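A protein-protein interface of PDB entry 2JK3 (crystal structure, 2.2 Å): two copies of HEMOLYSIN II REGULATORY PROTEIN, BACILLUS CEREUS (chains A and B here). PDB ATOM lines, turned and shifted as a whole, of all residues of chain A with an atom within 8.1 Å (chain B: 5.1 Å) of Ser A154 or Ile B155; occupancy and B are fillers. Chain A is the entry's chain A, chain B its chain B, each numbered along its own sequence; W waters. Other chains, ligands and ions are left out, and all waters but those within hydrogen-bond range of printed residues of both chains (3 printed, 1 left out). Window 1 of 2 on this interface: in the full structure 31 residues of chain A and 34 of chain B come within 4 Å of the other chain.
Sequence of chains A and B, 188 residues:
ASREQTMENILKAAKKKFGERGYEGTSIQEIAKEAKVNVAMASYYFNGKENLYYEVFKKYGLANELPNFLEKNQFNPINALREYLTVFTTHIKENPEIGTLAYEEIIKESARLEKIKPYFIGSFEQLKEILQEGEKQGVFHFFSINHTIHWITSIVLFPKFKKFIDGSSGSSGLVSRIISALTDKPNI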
ATOM      1  N   PHE A  88      27.687 -26.136  23.134  1.00  0.00           N
ATOM      2  CA  PHE A  88      27.867 -24.943  23.930  1.00  0.00           C
ATOM      3  C   PHE A  88      26.512 -24.413  24.515  1.00  0.00           C
ATOM      4  O   PHE A  88      26.355 -24.256  25.722  1.00  0.00           O
ATOM      5  CB  PHE A  88      28.533 -23.922  23.055  1.00  0.00           C
ATOM      6  CG  PHE A  88      29.030 -22.761  23.772  1.00  0.00           C
ATOM      7  CD1 PHE A  88      30.385 -22.437  23.736  1.00  0.00           C
ATOM      8  CD2 PHE A  88      28.162 -21.942  24.455  1.00  0.00           C
ATOM      9  CE1 PHE A  88      30.860 -21.318  24.397  1.00  0.00           C
ATOM     10  CE2 PHE A  88      28.630 -20.781  25.113  1.00  0.00           C
ATOM     11  CZ  PHE A  88      29.983 -20.479  25.086  1.00  0.00           C
ATOM     12  N   TYR A 103      28.159 -13.293  31.901  1.00  0.00           N
ATOM     13  CA  TYR A 103      27.864 -12.121  31.049  1.00  0.00           C
ATOM     14  C   TYR A 103      27.794 -10.818  31.885  1.00  0.00           C
ATOM     15  O   TYR A 103      28.239  -9.732  31.448  1.00  0.00           O
ATOM     16  CB  TYR A 103      26.569 -12.334  30.248  1.00  0.00           C
ATOM     17  CG  TYR A 103      26.568 -11.675  28.867  1.00  0.00           C
ATOM     18  CD1 TYR A 103      26.965 -12.378  27.739  1.00  0.00           C
ATOM     19  CD2 TYR A 103      26.176 -10.361  28.707  1.00  0.00           C
ATOM     20  CE1 TYR A 103      26.974 -11.793  26.503  1.00  0.00           C
ATOM     21  CE2 TYR A 103      26.161  -9.757  27.470  1.00  0.00           C
ATOM     22  CZ  TYR A 103      26.562 -10.484  26.364  1.00  0.00           C
ATOM     23  OH  TYR A 103      26.544  -9.891  25.127  1.00  0.00           O
ATOM     24  N   ILE A 106      31.291  -9.840  32.861  1.00  0.00           N
ATOM     25  CA  ILE A 106      31.921  -9.372  31.646  1.00  0.00           C
ATOM     26  C   ILE A 106      31.499  -7.945  31.297  1.00  0.00           C
ATOM     27  O   ILE A 106      32.352  -7.095  31.087  1.00  0.00           O
ATOM     28  CB  ILE A 106      31.560 -10.253  30.449  1.00  0.00           C
ATOM     29  CG1 ILE A 106      32.106 -11.669  30.606  1.00  0.00           C
ATOM     30  CG2 ILE A 106      32.042  -9.615  29.117  1.00  0.00           C
ATOM     31  CD1 ILE A 106      31.653 -12.575  29.496  1.00  0.00           C
ATOM     32  N   ILE A 107      30.199  -7.674  31.213  1.00  0.00           N
ATOM     33  CA  ILE A 107      29.784  -6.314  30.826  1.00  0.00           C
ATOM     34  C   ILE A 107      30.111  -5.284  31.895  1.00  0.00           C
ATOM     35  O   ILE A 107      30.232  -4.104  31.594  1.00  0.00           O
ATOM     36  CB  ILE A 107      28.286  -6.202  30.416  1.00  0.00           C
ATOM     37  CG1 ILE A 107      27.365  -6.439  31.620  1.00  0.00           C
ATOM     38  CG2 ILE A 107      28.013  -7.126  29.295  1.00  0.00           C
ATOM     39  CD1 ILE A 107      25.912  -6.149  31.332  1.00  0.00           C
ATOM     40  N   PHE A 124      36.410 -20.776  23.501  1.00  0.00           N
ATOM     41  CA  PHE A 124      36.581 -19.732  22.482  1.00  0.00           C
ATOM     42  C   PHE A 124      37.645 -20.168  21.516  1.00  0.00           C
ATOM     43  O   PHE A 124      37.551 -19.933  20.328  1.00  0.00           O
ATOM     44  CB  PHE A 124      36.946 -18.371  23.097  1.00  0.00           C
ATOM     45  CG  PHE A 124      35.897 -17.857  24.051  1.00  0.00           C
ATOM     46  CD1 PHE A 124      34.606 -18.355  23.982  1.00  0.00           C
ATOM     47  CD2 PHE A 124      36.199 -16.902  25.010  1.00  0.00           C
ATOM     48  CE1 PHE A 124      33.606 -17.885  24.882  1.00  0.00           C
ATOM     49  CE2 PHE A 124      35.246 -16.433  25.881  1.00  0.00           C
ATOM     50  CZ  PHE A 124      33.933 -16.934  25.818  1.00  0.00           C
ATOM     51  N   LEU A 127      36.218 -22.659  19.008  1.00  0.00           N
ATOM     52  CA  LEU A 127      35.482 -21.842  18.038  1.00  0.00           C
ATOM     53  C   LEU A 127      36.386 -21.206  17.004  1.00  0.00           C
ATOM     54  O   LEU A 127      36.105 -21.228  15.814  1.00  0.00           O
ATOM     55  CB  LEU A 127      34.692 -20.743  18.734  1.00  0.00           C
ATOM     56  CG  LEU A 127      33.869 -19.826  17.830  1.00  0.00           C
ATOM     57  CD1 LEU A 127      32.693 -20.599  17.214  1.00  0.00           C
ATOM     58  CD2 LEU A 127      33.365 -18.678  18.710  1.00  0.00           C
ATOM     59  N   HIS A 147      36.276 -10.329  14.852  1.00  0.00           N
ATOM     60  CA  HIS A 147      34.886  -9.810  14.850  1.00  0.00           C
ATOM     61  C   HIS A 147      33.877 -10.958  14.941  1.00  0.00           C
ATOM     62  O   HIS A 147      32.903 -10.925  15.705  1.00  0.00           O
ATOM     63  CB  HIS A 147      34.576  -8.886  13.642  1.00  0.00           C
ATOM     64  CG  HIS A 147      33.125  -8.497  13.583  1.00  0.00           C
ATOM     65  ND1 HIS A 147      32.587  -7.523  14.405  1.00  0.00           N
ATOM     66  CD2 HIS A 147      32.075  -9.038  12.906  1.00  0.00           C
ATOM     67  CE1 HIS A 147      31.282  -7.449  14.200  1.00  0.00           C
ATOM     68  NE2 HIS A 147      30.950  -8.335  13.276  1.00  0.00           N
ATOM     69  N   THR A 148      34.132 -12.029  14.208  1.00  0.00           N
ATOM     70  CA  THR A 148      33.140 -13.118  14.109  1.00  0.00           C
ATOM     71  C   THR A 148      33.019 -13.857  15.443  1.00  0.00           C
ATOM     72  O   THR A 148      31.930 -14.236  15.877  1.00  0.00           O
ATOM     73  CB  THR A 148      33.576 -14.118  12.998  1.00  0.00           C
ATOM     74  OG1 THR A 148      33.758 -13.439  11.768  1.00  0.00           O
ATOM     75  CG2 THR A 148      32.537 -15.209  12.750  1.00  0.00           C
ATOM     76  N   ILE A 149      34.160 -14.168  16.047  1.00  0.00           N
ATOM     77  CA  ILE A 149      34.180 -14.799  17.334  1.00  0.00           C
ATOM     78  C   ILE A 149      33.433 -13.924  18.373  1.00  0.00           C
ATOM     79  O   ILE A 149      32.621 -14.417  19.190  1.00  0.00           O
ATOM     80  CB  ILE A 149      35.627 -14.964  17.812  1.00  0.00           C
ATOM     81  CG1 ILE A 149      36.281 -16.133  17.096  1.00  0.00           C
ATOM     82  CG2 ILE A 149      35.676 -15.253  19.331  1.00  0.00           C
ATOM     83  CD1 ILE A 149      37.807 -16.068  17.217  1.00  0.00           C
ATOM     84  N   HIS A 150      33.721 -12.635  18.326  1.00  0.00           N
ATOM     85  CA  HIS A 150      32.994 -11.672  19.149  1.00  0.00           C
ATOM     86  C   HIS A 150      31.467 -11.730  19.041  1.00  0.00           C
ATOM     87  O   HIS A 150      30.793 -11.815  20.066  1.00  0.00           O
ATOM     88  CB  HIS A 150      33.527 -10.298  18.868  1.00  0.00           C
ATOM     89  CG  HIS A 150      32.837  -9.210  19.613  1.00  0.00           C
ATOM     90  ND1 HIS A 150      33.045  -7.879  19.321  1.00  0.00           N
ATOM     91  CD2 HIS A 150      31.918  -9.242  20.613  1.00  0.00           C
ATOM     92  CE1 HIS A 150      32.296  -7.136  20.122  1.00  0.00           C
ATOM     93  NE2 HIS A 150      31.612  -7.939  20.922  1.00  0.00           N
ATOM     94  N   TRP A 151      30.897 -11.704  17.830  1.00  0.00           N
ATOM     95  CA  TRP A 151      29.441 -11.675  17.761  1.00  0.00           C
ATOM     96  C   TRP A 151      28.868 -13.016  18.034  1.00  0.00           C
ATOM     97  O   TRP A 151      27.742 -13.120  18.533  1.00  0.00           O
ATOM     98  CB  TRP A 151      28.865 -11.040  16.470  1.00  0.00           C
ATOM     99  CG  TRP A 151      29.047 -11.728  15.157  1.00  0.00           C
ATOM    100  CD1 TRP A 151      29.948 -11.384  14.120  1.00  0.00           C
ATOM    101  CD2 TRP A 151      28.259 -12.817  14.657  1.00  0.00           C
ATOM    102  NE1 TRP A 151      29.770 -12.266  13.065  1.00  0.00           N
ATOM    103  CE2 TRP A 151      28.756 -13.155  13.376  1.00  0.00           C
ATOM    104  CE3 TRP A 151      27.222 -13.606  15.215  1.00  0.00           C
ATOM    105  CZ2 TRP A 151      28.170 -14.187  12.589  1.00  0.00           C
ATOM    106  CZ3 TRP A 151      26.705 -14.644  14.482  1.00  0.00           C
ATOM    107  CH2 TRP A 151      27.181 -14.935  13.173  1.00  0.00           C
ATOM    108  N   ILE A 152      29.612 -14.072  17.733  1.00  0.00           N
ATOM    109  CA  ILE A 152      29.048 -15.375  17.996  1.00  0.00           C
ATOM    110  C   ILE A 152      28.969 -15.619  19.511  1.00  0.00           C
ATOM    111  O   ILE A 152      27.921 -15.999  20.034  1.00  0.00           O
ATOM    112  CB  ILE A 152      29.847 -16.512  17.345  1.00  0.00           C
ATOM    113  CG1 ILE A 152      29.589 -16.531  15.827  1.00  0.00           C
ATOM    114  CG2 ILE A 152      29.362 -17.827  17.948  1.00  0.00           C
ATOM    115  CD1 ILE A 152      30.481 -17.515  15.019  1.00  0.00           C
ATOM    116  N   THR A 153      30.080 -15.388  20.219  1.00  0.00           N
ATOM    117  CA  THR A 153      30.063 -15.631  21.661  1.00  0.00           C
ATOM    118  C   THR A 153      29.148 -14.626  22.361  1.00  0.00           C
ATOM    119  O   THR A 153      28.511 -14.952  23.347  1.00  0.00           O
ATOM    120  CB  THR A 153      31.460 -15.597  22.248  1.00  0.00           C
ATOM    121  OG1 THR A 153      32.033 -14.290  22.065  1.00  0.00           O
ATOM    122  CG2 THR A 153      32.343 -16.662  21.565  1.00  0.00           C
ATOM    123  N   SER A 154      29.060 -13.403  21.836  1.00  0.00           N
ATOM    124  CA  SER A 154      28.168 -12.445  22.456  1.00  0.00           C
ATOM    125  C   SER A 154      26.708 -12.912  22.454  1.00  0.00           C
ATOM    126  O   SER A 154      26.010 -12.776  23.461  1.00  0.00           O
ATOM    127  CB  SER A 154      28.290 -11.064  21.836  1.00  0.00           C
ATOM    128  OG  SER A 154      27.075 -10.384  22.063  1.00  0.00           O
ATOM    129  N   ILE A 155      26.226 -13.464  21.343  1.00  0.00           N
ATOM    130  CA  ILE A 155      24.815 -13.888  21.326  1.00  0.00           C
ATOM    131  C   ILE A 155      24.614 -15.277  21.958  1.00  0.00           C
ATOM    132  O   ILE A 155      23.544 -15.588  22.516  1.00  0.00           O
ATOM    133  CB  ILE A 155      24.183 -13.740  19.890  1.00  0.00           C
ATOM    134  CG1 ILE A 155      24.808 -14.740  18.887  1.00  0.00           C
ATOM    135  CG2 ILE A 155      24.508 -12.344  19.363  1.00  0.00           C
ATOM    136  CD1 ILE A 155      24.093 -14.857  17.550  1.00  0.00           C
ATOM    137  N   VAL A 156      25.632 -16.116  21.914  1.00  0.00           N
ATOM    138  CA  VAL A 156      25.469 -17.441  22.474  1.00  0.00           C
ATOM    139  C   VAL A 156      25.460 -17.357  23.988  1.00  0.00           C
ATOM    140  O   VAL A 156      24.785 -18.131  24.675  1.00  0.00           O
ATOM    141  CB  VAL A 156      26.604 -18.437  22.024  1.00  0.00           C
ATOM    142  CG1 VAL A 156      26.772 -19.538  23.044  1.00  0.00           C
ATOM    143  CG2 VAL A 156      26.257 -19.044  20.658  1.00  0.00           C
ATOM    144  N   LEU A 157      26.240 -16.437  24.539  1.00  0.00           N
ATOM    145  CA  LEU A 157      26.262 -16.374  26.019  1.00  0.00           C
ATOM    146  C   LEU A 157      25.116 -15.545  26.630  1.00  0.00           C
ATOM    147  O   LEU A 157      25.014 -15.405  27.855  1.00  0.00           O
ATOM    148  CB  LEU A 157      27.606 -15.863  26.512  1.00  0.00           C
ATOM    149  CG  LEU A 157      28.786 -16.837  26.527  1.00  0.00           C
ATOM    150  CD1 LEU A 157      30.087 -16.023  26.690  1.00  0.00           C
ATOM    151  CD2 LEU A 157      28.661 -17.830  27.651  1.00  0.00           C
ATOM    152  N   PHE A 158      24.279 -14.978  25.770  1.00  0.00           N
ATOM    153  CA  PHE A 158      23.184 -14.109  26.169  1.00  0.00           C
ATOM    154  C   PHE A 158      21.849 -14.538  25.502  1.00  0.00           C
ATOM    155  O   PHE A 158      21.189 -13.741  24.812  1.00  0.00           O
ATOM    156  CB  PHE A 158      23.517 -12.672  25.764  1.00  0.00           C
ATOM    157  CG  PHE A 158      22.667 -11.644  26.448  1.00  0.00           C
ATOM    158  CD1 PHE A 158      21.609 -12.037  27.279  1.00  0.00           C
ATOM    159  CD2 PHE A 158      22.903 -10.279  26.259  1.00  0.00           C
ATOM    160  CE1 PHE A 158      20.799 -11.089  27.896  1.00  0.00           C
ATOM    161  CE2 PHE A 158      22.089  -9.311  26.878  1.00  0.00           C
ATOM    162  CZ  PHE A 158      21.042  -9.709  27.696  1.00  0.00           C
ATOM    163  N   PRO A 159      21.442 -15.795  25.716  1.00  0.00           N
ATOM    164  CA  PRO A 159      20.228 -16.321  25.094  1.00  0.00           C
ATOM    165  C   PRO A 159      19.010 -15.416  25.268  1.00  0.00           C
ATOM    166  O   PRO A 159      18.193 -15.324  24.357  1.00  0.00           O
ATOM    167  CB  PRO A 159      19.962 -17.649  25.857  1.00  0.00           C
ATOM    168  CG  PRO A 159      20.846 -17.618  27.074  1.00  0.00           C
ATOM    169  CD  PRO A 159      22.067 -16.790  26.600  1.00  0.00           C
ATOM    170  N   LYS A 160      18.838 -14.806  26.445  1.00  0.00           N
ATOM    171  CA  LYS A 160      17.616 -14.036  26.687  1.00  0.00           C
ATOM    172  C   LYS A 160      17.537 -12.735  25.895  1.00  0.00           C
ATOM    173  O   LYS A 160      16.488 -12.161  25.770  1.00  0.00           O
ATOM    174  CB  LYS A 160      17.393 -13.760  28.170  1.00  0.00           C
ATOM    175  CG  LYS A 160      17.144 -14.998  28.954  1.00  0.00           C
ATOM    176  CD  LYS A 160      16.283 -14.728  30.124  1.00  0.00           C
ATOM    177  CE  LYS A 160      16.030 -16.010  30.879  1.00  0.00           C
ATOM    178  NZ  LYS A 160      15.201 -15.682  32.048  1.00  0.00           N
ATOM    179  N   PHE A 161      18.646 -12.273  25.350  1.00  0.00           N
ATOM    180  CA  PHE A 161      18.597 -11.012  24.643  1.00  0.00           C
ATOM    181  C   PHE A 161      17.788 -11.204  23.379  1.00  0.00           C
ATOM    182  O   PHE A 161      17.124 -10.293  22.903  1.00  0.00           O
ATOM    183  CB  PHE A 161      20.003 -10.531  24.303  1.00  0.00           C
ATOM    184  CG  PHE A 161      20.028  -9.205  23.625  1.00  0.00           C
ATOM    185  CD1 PHE A 161      19.641  -8.086  24.288  1.00  0.00           C
ATOM    186  CD2 PHE A 161      20.412  -9.095  22.302  1.00  0.00           C
ATOM    187  CE1 PHE A 161      19.667  -6.852  23.674  1.00  0.00           C
ATOM    188  CE2 PHE A 161      20.431  -7.877  21.677  1.00  0.00           C
ATOM    189  CZ  PHE A 161      20.063  -6.743  22.378  1.00  0.00           C
ATOM    190  N   LEU A 174      18.886 -20.529  16.575  1.00  0.00           N
ATOM    191  CA  LEU A 174      20.144 -19.763  16.678  1.00  0.00           C
ATOM    192  C   LEU A 174      21.333 -20.405  15.942  1.00  0.00           C
ATOM    193  O   LEU A 174      22.116 -19.752  15.227  1.00  0.00           O
ATOM    194  CB  LEU A 174      20.514 -19.599  18.146  1.00  0.00           C
ATOM    195  CG  LEU A 174      21.729 -18.682  18.280  1.00  0.00           C
ATOM    196  CD1 LEU A 174      21.308 -17.244  17.940  1.00  0.00           C
ATOM    197  CD2 LEU A 174      22.382 -18.762  19.644  1.00  0.00           C
ATOM    198  N   TRP B 151      22.759  -9.517  16.291  1.00  0.00           N
ATOM    199  CA  TRP B 151      24.092  -9.513  16.803  1.00  0.00           C
ATOM    200  C   TRP B 151      24.627  -8.106  16.838  1.00  0.00           C
ATOM    201  O   TRP B 151      25.508  -7.810  17.621  1.00  0.00           O
ATOM    202  CB  TRP B 151      25.056 -10.468  16.065  1.00  0.00           C
ATOM    203  CG  TRP B 151      25.321 -10.245  14.567  1.00  0.00           C
ATOM    204  CD1 TRP B 151      24.799 -10.997  13.528  1.00  0.00           C
ATOM    205  CD2 TRP B 151      26.237  -9.297  13.947  1.00  0.00           C
ATOM    206  NE1 TRP B 151      25.308 -10.538  12.322  1.00  0.00           N
ATOM    207  CE2 TRP B 151      26.206  -9.526  12.560  1.00  0.00           C
ATOM    208  CE3 TRP B 151      27.102  -8.305  14.443  1.00  0.00           C
ATOM    209  CZ2 TRP B 151      26.943  -8.750  11.650  1.00  0.00           C
ATOM    210  CZ3 TRP B 151      27.825  -7.551  13.545  1.00  0.00           C
ATOM    211  CH2 TRP B 151      27.752  -7.790  12.158  1.00  0.00           C
ATOM    212  N   ILE B 152      24.147  -7.239  15.960  1.00  0.00           N
ATOM    213  CA  ILE B 152      24.617  -5.845  16.045  1.00  0.00           C
ATOM    214  C   ILE B 152      24.172  -5.191  17.345  1.00  0.00           C
ATOM    215  O   ILE B 152      24.960  -4.564  18.026  1.00  0.00           O
ATOM    216  CB  ILE B 152      24.164  -4.962  14.863  1.00  0.00           C
ATOM    217  CG1 ILE B 152      24.880  -5.415  13.581  1.00  0.00           C
ATOM    218  CG2 ILE B 152      24.448  -3.446  15.165  1.00  0.00           C
ATOM    219  CD1 ILE B 152      24.433  -4.690  12.356  1.00  0.00           C
ATOM    220  N   THR B 153      22.903  -5.309  17.697  1.00  0.00           N
ATOM    221  CA  THR B 153      22.452  -4.579  18.883  1.00  0.00           C
ATOM    222  C   THR B 153      23.086  -5.178  20.139  1.00  0.00           C
ATOM    223  O   THR B 153      23.433  -4.479  21.077  1.00  0.00           O
ATOM    224  CB  THR B 153      20.911  -4.536  18.990  1.00  0.00           C
ATOM    225  OG1 THR B 153      20.382  -5.865  19.109  1.00  0.00           O
ATOM    226  CG2 THR B 153      20.320  -3.888  17.751  1.00  0.00           C
ATOM    227  N   SER B 154      23.258  -6.491  20.117  1.00  0.00           N
ATOM    228  CA  SER B 154      23.933  -7.215  21.173  1.00  0.00           C
ATOM    229  C   SER B 154      25.370  -6.716  21.444  1.00  0.00           C
ATOM    230  O   SER B 154      25.784  -6.520  22.594  1.00  0.00           O
ATOM    231  CB  SER B 154      23.938  -8.686  20.792  1.00  0.00           C
ATOM    232  OG  SER B 154      24.398  -9.515  21.845  1.00  0.00           O
ATOM    233  N   ILE B 155      26.157  -6.523  20.408  1.00  0.00           N
ATOM    234  CA  ILE B 155      27.521  -6.084  20.658  1.00  0.00           C
ATOM    235  C   ILE B 155      27.619  -4.585  20.874  1.00  0.00           C
ATOM    236  O   ILE B 155      28.548  -4.144  21.551  1.00  0.00           O
ATOM    237  CB  ILE B 155      28.565  -6.583  19.570  1.00  0.00           C
ATOM    238  CG1 ILE B 155      28.312  -5.999  18.187  1.00  0.00           C
ATOM    239  CG2 ILE B 155      28.520  -8.088  19.417  1.00  0.00           C
ATOM    240  CD1 ILE B 155      29.429  -6.449  17.119  1.00  0.00           C
ATOM    241  N   VAL B 156      26.689  -3.781  20.341  1.00  0.00           N
ATOM    242  CA  VAL B 156      26.770  -2.307  20.575  1.00  0.00           C
ATOM    243  C   VAL B 156      26.283  -1.875  21.976  1.00  0.00           C
ATOM    244  O   VAL B 156      26.755  -0.891  22.563  1.00  0.00           O
ATOM    245  CB  VAL B 156      26.030  -1.450  19.496  1.00  0.00           C
ATOM    246  CG1 VAL B 156      26.547  -1.779  18.105  1.00  0.00           C
ATOM    247  CG2 VAL B 156      24.505  -1.638  19.559  1.00  0.00           C
ATOM    248  N   LEU B 157      25.343  -2.640  22.503  1.00  0.00           N
ATOM    249  CA  LEU B 157      24.693  -2.326  23.747  1.00  0.00           C
ATOM    250  C   LEU B 157      25.541  -2.812  24.954  1.00  0.00           C
ATOM    251  O   LEU B 157      25.302  -2.409  26.071  1.00  0.00           O
ATOM    252  CB  LEU B 157      23.326  -3.004  23.700  1.00  0.00           C
ATOM    253  CG  LEU B 157      22.303  -3.051  24.818  1.00  0.00           C
ATOM    254  CD1 LEU B 157      22.101  -1.673  25.412  1.00  0.00           C
ATOM    255  CD2 LEU B 157      20.992  -3.556  24.217  1.00  0.00           C
ATOM    256  N   PHE B 158      26.529  -3.677  24.711  1.00  0.00           N
ATOM    257  CA  PHE B 158      27.386  -4.229  25.766  1.00  0.00           C
ATOM    258  C   PHE B 158      28.836  -4.239  25.322  1.00  0.00           C
ATOM    259  O   PHE B 158      29.443  -5.275  25.138  1.00  0.00           O
ATOM    260  CB  PHE B 158      26.924  -5.623  26.124  1.00  0.00           C
ATOM    261  CG  PHE B 158      25.468  -5.675  26.469  1.00  0.00           C
ATOM    262  CD1 PHE B 158      25.005  -5.088  27.627  1.00  0.00           C
ATOM    263  CD2 PHE B 158      24.563  -6.254  25.607  1.00  0.00           C
ATOM    264  CE1 PHE B 158      23.647  -5.088  27.936  1.00  0.00           C
ATOM    265  CE2 PHE B 158      23.222  -6.290  25.906  1.00  0.00           C
ATOM    266  CZ  PHE B 158      22.759  -5.695  27.094  1.00  0.00           C
ATOM    267  N   PRO B 159      29.393  -3.062  25.115  1.00  0.00           N
ATOM    268  CA  PRO B 159      30.704  -2.949  24.498  1.00  0.00           C
ATOM    269  C   PRO B 159      31.868  -3.482  25.341  1.00  0.00           C
ATOM    270  O   PRO B 159      32.970  -3.650  24.827  1.00  0.00           O
ATOM    271  CB  PRO B 159      30.846  -1.430  24.298  1.00  0.00           C
ATOM    272  CG  PRO B 159      29.934  -0.830  25.328  1.00  0.00           C
ATOM    273  CD  PRO B 159      28.772  -1.747  25.363  1.00  0.00           C
ATOM    274  N   PHE B 161      31.967  -6.399  26.539  1.00  0.00           N
ATOM    275  CA  PHE B 161      32.134  -7.769  26.039  1.00  0.00           C
ATOM    276  C   PHE B 161      33.259  -7.852  25.010  1.00  0.00           C
ATOM    277  O   PHE B 161      34.071  -8.770  24.992  1.00  0.00           O
ATOM    278  CB  PHE B 161      30.825  -8.272  25.432  1.00  0.00           C
ATOM    279  CG  PHE B 161      30.817  -9.755  25.176  1.00  0.00           C
ATOM    280  CD1 PHE B 161      30.154 -10.618  26.039  1.00  0.00           C
ATOM    281  CD2 PHE B 161      31.487 -10.290  24.071  1.00  0.00           C
ATOM    282  CE1 PHE B 161      30.184 -12.015  25.804  1.00  0.00           C
ATOM    283  CE2 PHE B 161      31.506 -11.662  23.823  1.00  0.00           C
ATOM    284  CZ  PHE B 161      30.854 -12.525  24.690  1.00  0.00           C
ATOM    285  N   LEU B 174      35.063  -1.167  17.073  1.00  0.00           N
ATOM    286  CA  LEU B 174      33.765  -1.781  17.042  1.00  0.00           C
ATOM    287  C   LEU B 174      32.909  -1.355  15.838  1.00  0.00           C
ATOM    288  O   LEU B 174      32.263  -2.200  15.157  1.00  0.00           O
ATOM    289  CB  LEU B 174      33.025  -1.459  18.327  1.00  0.00           C
ATOM    290  CG  LEU B 174      31.622  -2.026  18.320  1.00  0.00           C
ATOM    291  CD1 LEU B 174      31.676  -3.552  18.181  1.00  0.00           C
ATOM    292  CD2 LEU B 174      30.922  -1.646  19.602  1.00  0.00           C
ATOM    293  N   ILE B 178      32.004  -3.644  12.439  1.00  0.00           N
ATOM    294  CA  ILE B 178      30.649  -4.019  12.079  1.00  0.00           C
ATOM    295  C   ILE B 178      30.466  -3.693  10.618  1.00  0.00           C
ATOM    296  O   ILE B 178      29.852  -4.454   9.879  1.00  0.00           O
ATOM    297  CB  ILE B 178      29.606  -3.285  12.892  1.00  0.00           C
ATOM    298  CG1 ILE B 178      29.633  -3.827  14.306  1.00  0.00           C
ATOM    299  CG2 ILE B 178      28.249  -3.431  12.237  1.00  0.00           C
ATOM    300  CD1 ILE B 178      28.824  -3.013  15.251  1.00  0.00           C
HETATM  301  O   HOH W   1      30.282  -6.117  22.758  1.00  0.00           O
HETATM  302  O   HOH W   2      22.481 -11.770  22.547  1.00  0.00           O
HETATM  303  O   HOH W   3      27.759  -8.117  23.591  1.00  0.00           O
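OG of Ser B154 lies within hydrogen-bond range of OG of Ser A154 (2.8 Å).
The side-chain hydroxyl of Ser A154 sits at hydrogen-bond distance from the side-chain hydroxyl of Tyr A103. The side-chain hydroxyl (OG1) of Thr A153 lies within hydrogen-bond range of the backbone carbonyl oxygen (O) of Ile A149, at 2.9 Å. O of His A150 is in hydrogen-bond range of OG1 of Thr A153 (3.4 Å).
Among the printed residues, merely in contact across the chains: Tyr A103 with Ser B154, Tyr A103 with Phe B161, Ile A106 with Phe B161, Ile A107 with Phe B158, His A147 with Trp B151, His A147 with Ile B155, His A147 with Ile B178, His A150 with Ile B155, His A150 with Phe B161, Trp A151 with Trp B151, Thr A153 with Phe B161, Ser A154 with Ile B155, Ser A154 with Phe B161, Ile A155 with Trp B151, Ile A155 with Ser B154, Phe A158 with Phe B158, Phe A161 with Thr B153, Phe A161 with Ser B154 and Phe A161 with Leu B157.
Printed residues of chain B within 4 Å of Ser A154: Ser B154, Ile B155 and Phe B161. Of chain A, only His A147 (3.6 Å), His A150 (3.4 Å) and Ser A154 (3.8 Å) come within 4 Å of Ile B155. Of chain A, only Tyr A103, Ser A154, Ile A155 and Phe A161 come within 4 Å of Ser B154. Of the printed residues of chain A, Phe B158 touches Ile A107 (3.7 Å) and Phe A158 (3.4 Å). Printed residues of chain B within 4 Å of Thr A153: Phe B161. Of the printed residues of chain A, Leu B157 touches Phe A161 (3.6 Å). Printed residues of chain B within 4 Å of Ile A106: Phe B161. Pro B159 touches none of the printed residues of chain A. The nearest printed residue of chain B that does not touch Ser A154 is Trp B151 (5.4 Å).
Of the 22 printed residues of chain A, 11 touch a printed residue of chain B. Printed residues of chain A that touch a printed residue of chain B: Tyr A103, Ile A106, Ile A107, His A147, His A150, Trp A151, Thr A153, Ser A154, Ile A155, Phe A158 and Phe A161. Hydrophobic or aromatic side chains of chain A within 4 Å of the printed part of chain B: Tyr A103, Ile A106, Ile A107, His A147, His A150, Trp A151, Ile A155, Phe A158 and Phe A161. Among the printed residues, 20 pairs touch across the chains.
Trp A151 touches its own counterpart, Trp B151. Thr A153 touches Phe B161, and with the chains exchanged Phe A161 touches Thr B153. Ser A154 touches Phe B161, and with the chains exchanged Phe A161 touches Ser B154. Ile A155 touches Trp B151, but with the chains exchanged Trp A151 does not touch Ile B155 (4.1 Å). Positions printed for both chains: 151, 152, 153, 154, 155, 156, 157, 158, 159, 161 and 174. Of the 20 pairs that touch across the chains among the printed residues, 9 have their exchanged pair printed and touching as well.
Water W3 lies within hydrogen-bond range of OH of Tyr A103, O of Ser B154 and OG of Ser A154. Water W1 lies within hydrogen-bond range of the backbone carbonyl oxygen (O) of Phe B158 (2.7 Å), the backbone carbonyl oxygen (O) of Ile B155 (2.9 Å) and a ring nitrogen (NE2) of His A150 (2.9 Å). Water W2 bridges OG of Ser B154 (3.0 Å) and O of Phe A158 (3.3 Å).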
